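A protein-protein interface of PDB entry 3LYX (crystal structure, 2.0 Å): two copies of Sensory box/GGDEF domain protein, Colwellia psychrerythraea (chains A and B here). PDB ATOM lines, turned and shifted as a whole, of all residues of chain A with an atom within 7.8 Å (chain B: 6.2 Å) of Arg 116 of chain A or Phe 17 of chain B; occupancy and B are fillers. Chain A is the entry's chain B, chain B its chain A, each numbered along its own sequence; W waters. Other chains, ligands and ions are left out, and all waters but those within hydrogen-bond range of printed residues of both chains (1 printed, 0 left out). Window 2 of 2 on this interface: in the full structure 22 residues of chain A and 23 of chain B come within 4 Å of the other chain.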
ATOM      1  N   VAL A  16      -2.800  36.602 -14.759  1.00  0.00           N
ATOM      2  CA  VAL A  16      -3.596  35.716 -15.602  1.00  0.00           C
ATOM      3  C   VAL A  16      -3.175  34.250 -15.443  1.00  0.00           C
ATOM      4  O   VAL A  16      -2.061  33.954 -15.006  1.00  0.00           O
ATOM      5  CB  VAL A  16      -3.482  36.120 -17.097  1.00  0.00           C
ATOM      6  CG1 VAL A  16      -4.027  37.535 -17.299  1.00  0.00           C
ATOM      7  CG2 VAL A  16      -2.016  36.043 -17.555  1.00  0.00           C
ATOM      8  N   PHE A  17      -4.072  33.334 -15.787  1.00  0.00           N
ATOM      9  CA  PHE A  17      -3.781  31.911 -15.692  1.00  0.00           C
ATOM     10  C   PHE A  17      -3.006  31.501 -16.939  1.00  0.00           C
ATOM     11  O   PHE A  17      -2.300  30.495 -16.949  1.00  0.00           O
ATOM     12  CB  PHE A  17      -5.077  31.109 -15.598  1.00  0.00           C
ATOM     13  CG  PHE A  17      -4.871  29.619 -15.581  1.00  0.00           C
ATOM     14  CD1 PHE A  17      -4.109  29.015 -14.581  1.00  0.00           C
ATOM     15  CD2 PHE A  17      -5.455  28.814 -16.559  1.00  0.00           C
ATOM     16  CE1 PHE A  17      -3.931  27.624 -14.552  1.00  0.00           C
ATOM     17  CE2 PHE A  17      -5.285  27.425 -16.542  1.00  0.00           C
ATOM     18  CZ  PHE A  17      -4.519  26.828 -15.533  1.00  0.00           C
ATOM     19  N   ASP A  18      -3.172  32.288 -17.993  1.00  0.00           N
ATOM     20  CA  ASP A  18      -2.484  32.062 -19.256  1.00  0.00           C
ATOM     21  C   ASP A  18      -0.974  32.137 -19.065  1.00  0.00           C
ATOM     22  O   ASP A  18      -0.481  33.010 -18.363  1.00  0.00           O
ATOM     23  CB  ASP A  18      -2.886  33.139 -20.260  1.00  0.00           C
ATOM     24  CG  ASP A  18      -4.358  33.098 -20.595  1.00  0.00           C
ATOM     25  OD1 ASP A  18      -4.688  32.537 -21.663  1.00  0.00           O
ATOM     26  OD2 ASP A  18      -5.173  33.619 -19.783  1.00  0.00           O
ATOM     27  N   ALA A  19      -0.244  31.230 -19.698  1.00  0.00           N
ATOM     28  CA  ALA A  19       1.214  31.258 -19.618  1.00  0.00           C
ATOM     29  C   ALA A  19       1.697  32.115 -20.785  1.00  0.00           C
ATOM     30  O   ALA A  19       1.563  31.733 -21.958  1.00  0.00           O
ATOM     31  CB  ALA A  19       1.767  29.851 -19.734  1.00  0.00           C
ATOM     32  N   ILE A  20       2.227  33.290 -20.465  1.00  0.00           N
ATOM     33  CA  ILE A  20       2.738  34.201 -21.478  1.00  0.00           C
ATOM     34  C   ILE A  20       4.250  34.014 -21.604  1.00  0.00           C
ATOM     35  O   ILE A  20       4.965  34.008 -20.601  1.00  0.00           O
ATOM     36  CB  ILE A  20       2.483  35.683 -21.102  1.00  0.00           C
ATOM     37  CG1 ILE A  20       0.989  35.923 -20.838  1.00  0.00           C
ATOM     38  CG2 ILE A  20       2.966  36.600 -22.225  1.00  0.00           C
ATOM     39  CD1 ILE A  20       0.107  35.609 -22.021  1.00  0.00           C
ATOM     40  N   LEU A  39       2.754  26.531 -15.536  1.00  0.00           N
ATOM     41  CA  LEU A  39       2.608  25.566 -16.620  1.00  0.00           C
ATOM     42  C   LEU A  39       3.854  24.765 -16.969  1.00  0.00           C
ATOM     43  O   LEU A  39       3.799  23.539 -17.068  1.00  0.00           O
ATOM     44  CB  LEU A  39       2.114  26.266 -17.883  1.00  0.00           C
ATOM     45  CG  LEU A  39       1.956  25.409 -19.140  1.00  0.00           C
ATOM     46  CD1 LEU A  39       0.838  24.377 -18.950  1.00  0.00           C
ATOM     47  CD2 LEU A  39       1.637  26.320 -20.301  1.00  0.00           C
ATOM     48  N   TYR A  40       4.970  25.464 -17.158  1.00  0.00           N
ATOM     49  CA  TYR A  40       6.217  24.828 -17.561  1.00  0.00           C
ATOM     50  C   TYR A  40       7.118  24.351 -16.429  1.00  0.00           C
ATOM     51  O   TYR A  40       7.939  23.443 -16.628  1.00  0.00           O
ATOM     52  CB  TYR A  40       6.998  25.782 -18.470  1.00  0.00           C
ATOM     53  CG  TYR A  40       6.291  26.103 -19.771  1.00  0.00           C
ATOM     54  CD1 TYR A  40       6.136  25.134 -20.760  1.00  0.00           C
ATOM     55  CD2 TYR A  40       5.755  27.377 -20.006  1.00  0.00           C
ATOM     56  CE1 TYR A  40       5.456  25.426 -21.963  1.00  0.00           C
ATOM     57  CE2 TYR A  40       5.085  27.679 -21.191  1.00  0.00           C
ATOM     58  CZ  TYR A  40       4.938  26.697 -22.163  1.00  0.00           C
ATOM     59  OH  TYR A  40       4.274  26.985 -23.336  1.00  0.00           O
ATOM     60  N   GLY A  80      -1.858  26.304 -32.547  1.00  0.00           N
ATOM     61  CA  GLY A  80      -1.709  24.872 -32.705  1.00  0.00           C
ATOM     62  C   GLY A  80      -1.685  24.181 -31.363  1.00  0.00           C
ATOM     63  O   GLY A  80      -1.561  24.832 -30.332  1.00  0.00           O
ATOM     64  N   GLU A  81      -1.835  22.863 -31.382  1.00  0.00           N
ATOM     65  CA  GLU A  81      -1.810  22.054 -30.173  1.00  0.00           C
ATOM     66  C   GLU A  81      -0.541  21.245 -30.299  1.00  0.00           C
ATOM     67  O   GLU A  81      -0.433  20.363 -31.151  1.00  0.00           O
ATOM     68  CB  GLU A  81      -3.027  21.139 -30.120  1.00  0.00           C
ATOM     69  CG  GLU A  81      -4.304  21.851 -29.716  1.00  0.00           C
ATOM     70  CD  GLU A  81      -5.530  21.000 -29.962  1.00  0.00           C
ATOM     71  OE1 GLU A  81      -5.487  19.785 -29.680  1.00  0.00           O
ATOM     72  OE2 GLU A  81      -6.541  21.550 -30.437  1.00  0.00           O
ATOM     73  N   ILE A  82       0.425  21.564 -29.450  1.00  0.00           N
ATOM     74  CA  ILE A  82       1.728  20.924 -29.495  1.00  0.00           C
ATOM     75  C   ILE A  82       2.116  20.270 -28.177  1.00  0.00           C
ATOM     76  O   ILE A  82       1.495  20.517 -27.146  1.00  0.00           O
ATOM     77  CB  ILE A  82       2.794  21.979 -29.858  1.00  0.00           C
ATOM     78  CG1 ILE A  82       2.742  23.125 -28.835  1.00  0.00           C
ATOM     79  CG2 ILE A  82       2.524  22.533 -31.264  1.00  0.00           C
ATOM     80  CD1 ILE A  82       3.791  24.201 -29.040  1.00  0.00           C
ATOM     81  N   MET A  84       4.494  19.539 -24.893  1.00  0.00           N
ATOM     82  CA  MET A  84       5.181  20.418 -23.967  1.00  0.00           C
ATOM     83  C   MET A  84       6.109  19.565 -23.100  1.00  0.00           C
ATOM     84  O   MET A  84       5.756  18.447 -22.719  1.00  0.00           O
ATOM     85  CB  MET A  84       4.120  21.113 -23.110  1.00  0.00           C
ATOM     86  CG  MET A  84       4.626  22.035 -22.040  1.00  0.00           C
ATOM     87  SD  MET A  84       3.421  22.136 -20.706  1.00  0.00           S
ATOM     88  CE  MET A  84       4.279  21.122 -19.490  1.00  0.00           C
ATOM     89  N   TRP A  93       0.453  18.173 -23.383  1.00  0.00           N
ATOM     90  CA  TRP A  93       0.005  18.913 -24.558  1.00  0.00           C
ATOM     91  C   TRP A  93      -0.555  20.255 -24.122  1.00  0.00           C
ATOM     92  O   TRP A  93      -1.126  20.376 -23.039  1.00  0.00           O
ATOM     93  CB  TRP A  93      -1.070  18.144 -25.335  1.00  0.00           C
ATOM     94  CG  TRP A  93      -0.569  16.928 -26.039  1.00  0.00           C
ATOM     95  CD1 TRP A  93      -0.354  15.693 -25.499  1.00  0.00           C
ATOM     96  CD2 TRP A  93      -0.185  16.836 -27.414  1.00  0.00           C
ATOM     97  NE1 TRP A  93       0.139  14.837 -26.452  1.00  0.00           N
ATOM     98  CE2 TRP A  93       0.256  15.513 -27.637  1.00  0.00           C
ATOM     99  CE3 TRP A  93      -0.168  17.745 -28.482  1.00  0.00           C
ATOM    100  CZ2 TRP A  93       0.712  15.076 -28.884  1.00  0.00           C
ATOM    101  CZ3 TRP A  93       0.285  17.310 -29.720  1.00  0.00           C
ATOM    102  CH2 TRP A  93       0.719  15.987 -29.910  1.00  0.00           C
ATOM    103  N   ILE A  94      -0.384  21.262 -24.973  1.00  0.00           N
ATOM    104  CA  ILE A  94      -0.872  22.603 -24.683  1.00  0.00           C
ATOM    105  C   ILE A  94      -1.513  23.208 -25.922  1.00  0.00           C
ATOM    106  O   ILE A  94      -1.214  22.814 -27.050  1.00  0.00           O
ATOM    107  CB  ILE A  94       0.275  23.546 -24.261  1.00  0.00           C
ATOM    108  CG1 ILE A  94       1.363  23.549 -25.340  1.00  0.00           C
ATOM    109  CG2 ILE A  94       0.890  23.089 -22.946  1.00  0.00           C
ATOM    110  CD1 ILE A  94       2.486  24.532 -25.081  1.00  0.00           C
ATOM    111  N   GLU A  95      -2.419  24.147 -25.699  1.00  0.00           N
ATOM    112  CA  GLU A  95      -3.052  24.866 -26.791  1.00  0.00           C
ATOM    113  C   GLU A  95      -2.162  26.104 -26.829  1.00  0.00           C
ATOM    114  O   GLU A  95      -1.977  26.769 -25.809  1.00  0.00           O
ATOM    115  CB  GLU A  95      -4.494  25.248 -26.439  1.00  0.00           C
ATOM    116  CG  GLU A  95      -5.078  26.312 -27.364  1.00  0.00           C
ATOM    117  CD  GLU A  95      -6.585  26.440 -27.233  1.00  0.00           C
ATOM    118  OE1 GLU A  95      -7.084  26.527 -26.090  1.00  0.00           O
ATOM    119  OE2 GLU A  95      -7.270  26.454 -28.279  1.00  0.00           O
ATOM    120  N   SER A  96      -1.595  26.402 -27.989  1.00  0.00           N
ATOM    121  CA  SER A  96      -0.680  27.528 -28.087  1.00  0.00           C
ATOM    122  C   SER A  96      -0.967  28.478 -29.248  1.00  0.00           C
ATOM    123  O   SER A  96      -1.535  28.086 -30.273  1.00  0.00           O
ATOM    124  CB  SER A  96       0.759  26.987 -28.179  1.00  0.00           C
ATOM    125  OG  SER A  96       1.706  28.034 -28.300  1.00  0.00           O
ATOM    126  N   MET A  97      -0.567  29.730 -29.068  1.00  0.00           N
ATOM    127  CA  MET A  97      -0.751  30.763 -30.077  1.00  0.00           C
ATOM    128  C   MET A  97       0.495  31.639 -30.076  1.00  0.00           C
ATOM    129  O   MET A  97       1.091  31.884 -29.032  1.00  0.00           O
ATOM    130  CB  MET A  97      -1.977  31.607 -29.740  1.00  0.00           C
ATOM    131  CG  MET A  97      -2.279  32.723 -30.721  1.00  0.00           C
ATOM    132  SD  MET A  97      -3.359  33.942 -29.940  1.00  0.00           S
ATOM    133  CE  MET A  97      -2.158  34.838 -29.022  1.00  0.00           C
ATOM    134  N   ILE A 114       1.187  32.618 -26.192  1.00  0.00           N
ATOM    135  CA  ILE A 114       0.137  32.428 -25.181  1.00  0.00           C
ATOM    136  C   ILE A 114      -0.101  30.920 -25.117  1.00  0.00           C
ATOM    137  O   ILE A 114      -0.321  30.278 -26.145  1.00  0.00           O
ATOM    138  CB  ILE A 114      -1.197  33.140 -25.572  1.00  0.00           C
ATOM    139  CG1 ILE A 114      -1.005  34.656 -25.607  1.00  0.00           C
ATOM    140  CG2 ILE A 114      -2.288  32.812 -24.538  1.00  0.00           C
ATOM    141  CD1 ILE A 114      -0.005  35.128 -26.616  1.00  0.00           C
ATOM    142  N   ASN A 115      -0.071  30.349 -23.920  1.00  0.00           N
ATOM    143  CA  ASN A 115      -0.218  28.906 -23.804  1.00  0.00           C
ATOM    144  C   ASN A 115      -1.157  28.455 -22.682  1.00  0.00           C
ATOM    145  O   ASN A 115      -1.308  29.148 -21.676  1.00  0.00           O
ATOM    146  CB  ASN A 115       1.176  28.297 -23.590  1.00  0.00           C
ATOM    147  CG  ASN A 115       2.169  28.708 -24.670  1.00  0.00           C
ATOM    148  OD1 ASN A 115       2.307  28.031 -25.691  1.00  0.00           O
ATOM    149  ND2 ASN A 115       2.851  29.828 -24.456  1.00  0.00           N
ATOM    150  N   ARG A 116      -1.766  27.283 -22.867  1.00  0.00           N
ATOM    151  CA  ARG A 116      -2.685  26.695 -21.889  1.00  0.00           C
ATOM    152  C   ARG A 116      -2.621  25.168 -21.897  1.00  0.00           C
ATOM    153  O   ARG A 116      -2.707  24.532 -22.949  1.00  0.00           O
ATOM    154  CB  ARG A 116      -4.133  27.118 -22.166  1.00  0.00           C
ATOM    155  CG  ARG A 116      -4.492  28.529 -21.713  1.00  0.00           C
ATOM    156  CD  ARG A 116      -5.916  28.867 -22.123  1.00  0.00           C
ATOM    157  NE  ARG A 116      -6.075  28.846 -23.575  1.00  0.00           N
ATOM    158  CZ  ARG A 116      -5.647  29.805 -24.394  1.00  0.00           C
ATOM    159  NH1 ARG A 116      -5.032  30.878 -23.912  1.00  0.00           N
ATOM    160  NH2 ARG A 116      -5.824  29.686 -25.703  1.00  0.00           N
ATOM    161  N   ASP A 117      -2.489  24.586 -20.713  1.00  0.00           N
ATOM    162  CA  ASP A 117      -2.426  23.140 -20.566  1.00  0.00           C
ATOM    163  C   ASP A 117      -3.689  22.483 -21.101  1.00  0.00           C
ATOM    164  O   ASP A 117      -4.802  22.925 -20.819  1.00  0.00           O
ATOM    165  CB  ASP A 117      -2.236  22.763 -19.094  1.00  0.00           C
ATOM    166  CG  ASP A 117      -2.489  21.293 -18.837  1.00  0.00           C
ATOM    167  OD1 ASP A 117      -2.046  20.461 -19.658  1.00  0.00           O
ATOM    168  OD2 ASP A 117      -3.128  20.966 -17.813  1.00  0.00           O
ATOM    169  N   ILE A 118      -3.496  21.418 -21.870  1.00  0.00           N
ATOM    170  CA  ILE A 118      -4.592  20.679 -22.468  1.00  0.00           C
ATOM    171  C   ILE A 118      -4.339  19.176 -22.283  1.00  0.00           C
ATOM    172  O   ILE A 118      -5.128  18.336 -22.728  1.00  0.00           O
ATOM    173  CB  ILE A 118      -4.707  21.056 -23.979  1.00  0.00           C
ATOM    174  CG1 ILE A 118      -6.104  21.588 -24.272  1.00  0.00           C
ATOM    175  CG2 ILE A 118      -4.347  19.877 -24.874  1.00  0.00           C
ATOM    176  CD1 ILE A 118      -6.415  22.868 -23.549  1.00  0.00           C
ATOM    177  N   THR A 119      -3.237  18.859 -21.603  1.00  0.00           N
ATOM    178  CA  THR A 119      -2.823  17.478 -21.349  1.00  0.00           C
ATOM    179  C   THR A 119      -3.997  16.556 -21.031  1.00  0.00           C
ATOM    180  O   THR A 119      -4.240  15.586 -21.752  1.00  0.00           O
ATOM    181  CB  THR A 119      -1.794  17.402 -20.193  1.00  0.00           C
ATOM    182  OG1 THR A 119      -2.397  17.875 -18.981  1.00  0.00           O
ATOM    183  CG2 THR A 119      -0.568  18.251 -20.510  1.00  0.00           C
ATOM    184  N   TYR B  15      -5.035  38.993 -26.156  1.00  0.00           N
ATOM    185  CA  TYR B  15      -4.689  37.692 -26.719  1.00  0.00           C
ATOM    186  C   TYR B  15      -4.936  36.569 -25.712  1.00  0.00           C
ATOM    187  O   TYR B  15      -5.202  35.430 -26.093  1.00  0.00           O
ATOM    188  CB  TYR B  15      -3.224  37.686 -27.180  1.00  0.00           C
ATOM    189  CG  TYR B  15      -2.972  38.498 -28.434  1.00  0.00           C
ATOM    190  CD1 TYR B  15      -3.322  38.003 -29.699  1.00  0.00           C
ATOM    191  CD2 TYR B  15      -2.410  39.769 -28.360  1.00  0.00           C
ATOM    192  CE1 TYR B  15      -3.111  38.768 -30.857  1.00  0.00           C
ATOM    193  CE2 TYR B  15      -2.201  40.536 -29.502  1.00  0.00           C
ATOM    194  CZ  TYR B  15      -2.552  40.030 -30.744  1.00  0.00           C
ATOM    195  OH  TYR B  15      -2.344  40.797 -31.865  1.00  0.00           O
ATOM    196  N   VAL B  16      -4.881  36.887 -24.424  1.00  0.00           N
ATOM    197  CA  VAL B  16      -5.103  35.862 -23.403  1.00  0.00           C
ATOM    198  C   VAL B  16      -6.547  35.373 -23.362  1.00  0.00           C
ATOM    199  O   VAL B  16      -7.467  36.082 -23.777  1.00  0.00           O
ATOM    200  CB  VAL B  16      -4.718  36.376 -21.993  1.00  0.00           C
ATOM    201  CG1 VAL B  16      -3.232  36.683 -21.948  1.00  0.00           C
ATOM    202  CG2 VAL B  16      -5.533  37.625 -21.652  1.00  0.00           C
ATOM    203  N   PHE B  17      -6.735  34.154 -22.868  1.00  0.00           N
ATOM    204  CA  PHE B  17      -8.066  33.569 -22.744  1.00  0.00           C
ATOM    205  C   PHE B  17      -8.762  34.117 -21.495  1.00  0.00           C
ATOM    206  O   PHE B  17      -9.985  34.221 -21.453  1.00  0.00           O
ATOM    207  CB  PHE B  17      -7.963  32.044 -22.661  1.00  0.00           C
ATOM    208  CG  PHE B  17      -9.299  31.336 -22.623  1.00  0.00           C
ATOM    209  CD1 PHE B  17     -10.301  31.648 -23.544  1.00  0.00           C
ATOM    210  CD2 PHE B  17      -9.537  30.328 -21.697  1.00  0.00           C
ATOM    211  CE1 PHE B  17     -11.515  30.964 -23.543  1.00  0.00           C
ATOM    212  CE2 PHE B  17     -10.749  29.636 -21.687  1.00  0.00           C
ATOM    213  CZ  PHE B  17     -11.740  29.957 -22.615  1.00  0.00           C
ATOM    214  N   ASP B  18      -7.979  34.466 -20.474  1.00  0.00           N
ATOM    215  CA  ASP B  18      -8.542  35.016 -19.242  1.00  0.00           C
ATOM    216  C   ASP B  18      -9.275  36.337 -19.520  1.00  0.00           C
ATOM    217  O   ASP B  18      -8.825  37.157 -20.323  1.00  0.00           O
ATOM    218  CB  ASP B  18      -7.430  35.244 -18.201  1.00  0.00           C
ATOM    219  CG  ASP B  18      -7.130  33.997 -17.372  1.00  0.00           C
ATOM    220  OD1 ASP B  18      -7.579  32.897 -17.749  1.00  0.00           O
ATOM    221  OD2 ASP B  18      -6.444  34.117 -16.338  1.00  0.00           O
ATOM    222  N   ALA B  19     -10.407  36.532 -18.848  1.00  0.00           N
ATOM    223  CA  ALA B  19     -11.204  37.748 -19.020  1.00  0.00           C
ATOM    224  C   ALA B  19     -10.720  38.813 -18.034  1.00  0.00           C
ATOM    225  O   ALA B  19     -10.850  38.649 -16.813  1.00  0.00           O
ATOM    226  CB  ALA B  19     -12.698  37.433 -18.787  1.00  0.00           C
ATOM    227  N   ASN B  33     -10.885  43.595 -21.979  1.00  0.00           N
ATOM    228  CA  ASN B  33     -10.134  42.875 -23.018  1.00  0.00           C
ATOM    229  C   ASN B  33     -11.004  41.906 -23.822  1.00  0.00           C
ATOM    230  O   ASN B  33     -12.183  41.711 -23.516  1.00  0.00           O
ATOM    231  CB  ASN B  33      -8.930  42.126 -22.401  1.00  0.00           C
ATOM    232  CG  ASN B  33      -9.325  40.843 -21.683  1.00  0.00           C
ATOM    233  OD1 ASN B  33     -10.445  40.714 -21.197  1.00  0.00           O
ATOM    234  ND2 ASN B  33      -8.386  39.892 -21.592  1.00  0.00           N
ATOM    235  N   GLY B  35     -10.885  38.733 -23.943  1.00  0.00           N
ATOM    236  CA  GLY B  35     -11.279  37.571 -23.173  1.00  0.00           C
ATOM    237  C   GLY B  35     -12.590  37.844 -22.458  1.00  0.00           C
ATOM    238  O   GLY B  35     -13.448  36.960 -22.343  1.00  0.00           O
ATOM    239  N   SER B  36     -12.743  39.077 -21.980  1.00  0.00           N
ATOM    240  CA  SER B  36     -13.947  39.486 -21.272  1.00  0.00           C
ATOM    241  C   SER B  36     -15.124  39.568 -22.240  1.00  0.00           C
ATOM    242  O   SER B  36     -16.256  39.256 -21.884  1.00  0.00           O
ATOM    243  CB  SER B  36     -13.709  40.823 -20.572  1.00  0.00           C
ATOM    244  OG  SER B  36     -12.818  40.640 -19.473  1.00  0.00           O
ATOM    245  N   THR B  38     -15.558  37.643 -24.689  1.00  0.00           N
ATOM    246  CA  THR B  38     -15.957  36.255 -24.920  1.00  0.00           C
ATOM    247  C   THR B  38     -16.742  35.676 -23.743  1.00  0.00           C
ATOM    248  O   THR B  38     -17.791  35.051 -23.923  1.00  0.00           O
ATOM    249  CB  THR B  38     -14.716  35.368 -25.164  1.00  0.00           C
ATOM    250  OG1 THR B  38     -13.964  35.888 -26.265  1.00  0.00           O
ATOM    251  CG2 THR B  38     -15.115  33.950 -25.466  1.00  0.00           C
ATOM    252  N   ASN B 115     -10.828  36.792 -14.681  1.00  0.00           N
ATOM    253  CA  ASN B 115     -11.908  35.813 -14.616  1.00  0.00           C
ATOM    254  C   ASN B 115     -11.841  34.687 -15.646  1.00  0.00           C
ATOM    255  O   ASN B 115     -11.361  34.880 -16.759  1.00  0.00           O
ATOM    256  CB  ASN B 115     -13.237  36.570 -14.777  1.00  0.00           C
ATOM    257  CG  ASN B 115     -13.313  37.801 -13.891  1.00  0.00           C
ATOM    258  OD1 ASN B 115     -13.869  37.756 -12.794  1.00  0.00           O
ATOM    259  ND2 ASN B 115     -12.736  38.909 -14.358  1.00  0.00           N
ATOM    260  N   ARG B 116     -12.336  33.511 -15.263  1.00  0.00           N
ATOM    261  CA  ARG B 116     -12.367  32.344 -16.147  1.00  0.00           C
ATOM    262  C   ARG B 116     -13.638  31.555 -15.923  1.00  0.00           C
ATOM    263  O   ARG B 116     -14.076  31.384 -14.793  1.00  0.00           O
ATOM    264  CB  ARG B 116     -11.194  31.406 -15.878  1.00  0.00           C
ATOM    265  CG  ARG B 116      -9.877  31.863 -16.428  1.00  0.00           C
ATOM    266  CD  ARG B 116      -8.789  30.934 -15.922  1.00  0.00           C
ATOM    267  NE  ARG B 116      -8.790  30.905 -14.468  1.00  0.00           N
ATOM    268  CZ  ARG B 116      -8.413  31.922 -13.701  1.00  0.00           C
ATOM    269  NH1 ARG B 116      -7.990  33.055 -14.248  1.00  0.00           N
ATOM    270  NH2 ARG B 116      -8.469  31.810 -12.384  1.00  0.00           N
ATOM    271  N   ASP B 117     -14.214  31.059 -17.010  1.00  0.00           N
ATOM    272  CA  ASP B 117     -15.438  30.274 -16.933  1.00  0.00           C
ATOM    273  C   ASP B 117     -15.209  28.869 -16.370  1.00  0.00           C
ATOM    274  O   ASP B 117     -14.256  28.185 -16.745  1.00  0.00           O
ATOM    275  CB  ASP B 117     -16.068  30.182 -18.323  1.00  0.00           C
ATOM    276  CG  ASP B 117     -17.343  29.364 -18.333  1.00  0.00           C
ATOM    277  OD1 ASP B 117     -18.123  29.474 -17.366  1.00  0.00           O
ATOM    278  OD2 ASP B 117     -17.571  28.623 -19.312  1.00  0.00           O
HETATM  279  O   HOH W   1      -6.132  35.349 -28.996  1.00  0.00           O
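Water W1 bridges the backbone carbonyl oxygen (O) of Tyr 15 of chain B (3.0 Å) and the side-chain sulfur (SD) of Met 97 of chain A (3.2 Å).
Hydrophobic or aromatic side chains of chain A within 4 Å of the printed part of chain B: Val 16, Phe 17, Ile 20 and Met 97.
Printed residues of chain B that touch a printed residue of chain A: Tyr 15, Val 16, Phe 17, Asp 18 and Arg 116.
Hydrophobic or aromatic side chains of chain B within 4 Å of the printed part of chain A: Tyr 15, Val 16 and Phe 17.
Among the printed residues, no Asp or Glu carboxylate lies within 4 Å of a Lys or Arg side-chain nitrogen of the other chain.
Val 16 of chain A touches Asp 18 of chain B, and with the chains exchanged Asp 18 of chain A touches Val 16 of chain B.
Phe 17 of chain A touches Asp 18 of chain B, and with the chains exchanged Asp 18 of chain A touches Phe 17 of chain B.
Phe 17 of chain A touches Arg 116 of chain B, and with the chains exchanged Arg 116 of chain A touches Phe 17 of chain B.
Asp 18 of chain B touches its own counterpart, Asp 18 of chain A.
Positions printed for both chains: 16, 17, 18, 19, 115, 116 and 117.
Of the 9 pairs that touch across the chains among the printed residues, 7 have their exchanged pair printed and touching as well.
The backbone NH (N) of Phe 17 of chain B sits at hydrogen-bond distance from the side-chain carboxylate (OD1) of Asp 18 of chain A (2.9 Å).
The side-chain carboxylate (OD2) of Asp 18 of chain B sits at hydrogen-bond distance from the backbone NH (N) of Phe 17 of chain A, 2.6 Å away.
N of Asp 18 of chain B is in hydrogen-bond range of OD2 of Asp 18 of chain A, at 3.0 Å.
O of Asp 18 of chain B sits at hydrogen-bond distance from ND2 of Asn 33 of chain B, 3.0 Å away.
OD2 of Asp 18 of chain B lies within salt-bridge range of NH1 of Arg 116 of chain B (2.8 Å).
OD1 of Asp 18 of chain A lies within salt-bridge range of NH1 of Arg 116 of chain A (2.8 Å).
The side-chain carboxylate of Glu 95 of chain A lies within salt-bridge range of the guanidinium group of Arg 116 of chain A (3.4 Å).
The backbone carbonyl oxygen (O) of Met 97 of chain A lies within hydrogen-bond range of the backbone NH (N) of Ile 114 of chain A (2.9 Å).
Asp 18 of chain B touches Val 16 of chain A (OD2 to CA, 3.3 Å).
Phe 17 of chain A touches Arg 116 of chain B.
Val 16 of chain B touches Asp 18 of chain A.
Ile 20 of chain A touches Val 16 of chain B.
Tyr 15 of chain B touches Met 97 of chain A.
Arg 116 of chain A touches Phe 17 of chain B.
Printed residues of chain B within 4 Å of Asp 18 of chain A: Val 16, Phe 17 and Asp 18.
Ala 19 of chain A touches none of the printed residues of chain B.
Of the printed residues of chain B, Arg 116 of chain A touches Phe 17 (3.4 Å).
Printed residues of chain A within 4 Å of Tyr 15 of chain B: Met 97.
Of chain A, only Asp 18 (2.9 Å) and Arg 116 (3.4 Å) come within 4 Å of Phe 17 of chain B.
Printed residues of chain A within 4 Å of Asp 18 of chain B: Val 16, Phe 17 and Asp 18.
The nearest printed residue of chain B that does not touch Phe 17 of chain A is Phe 17 of chain B (6.7 Å).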
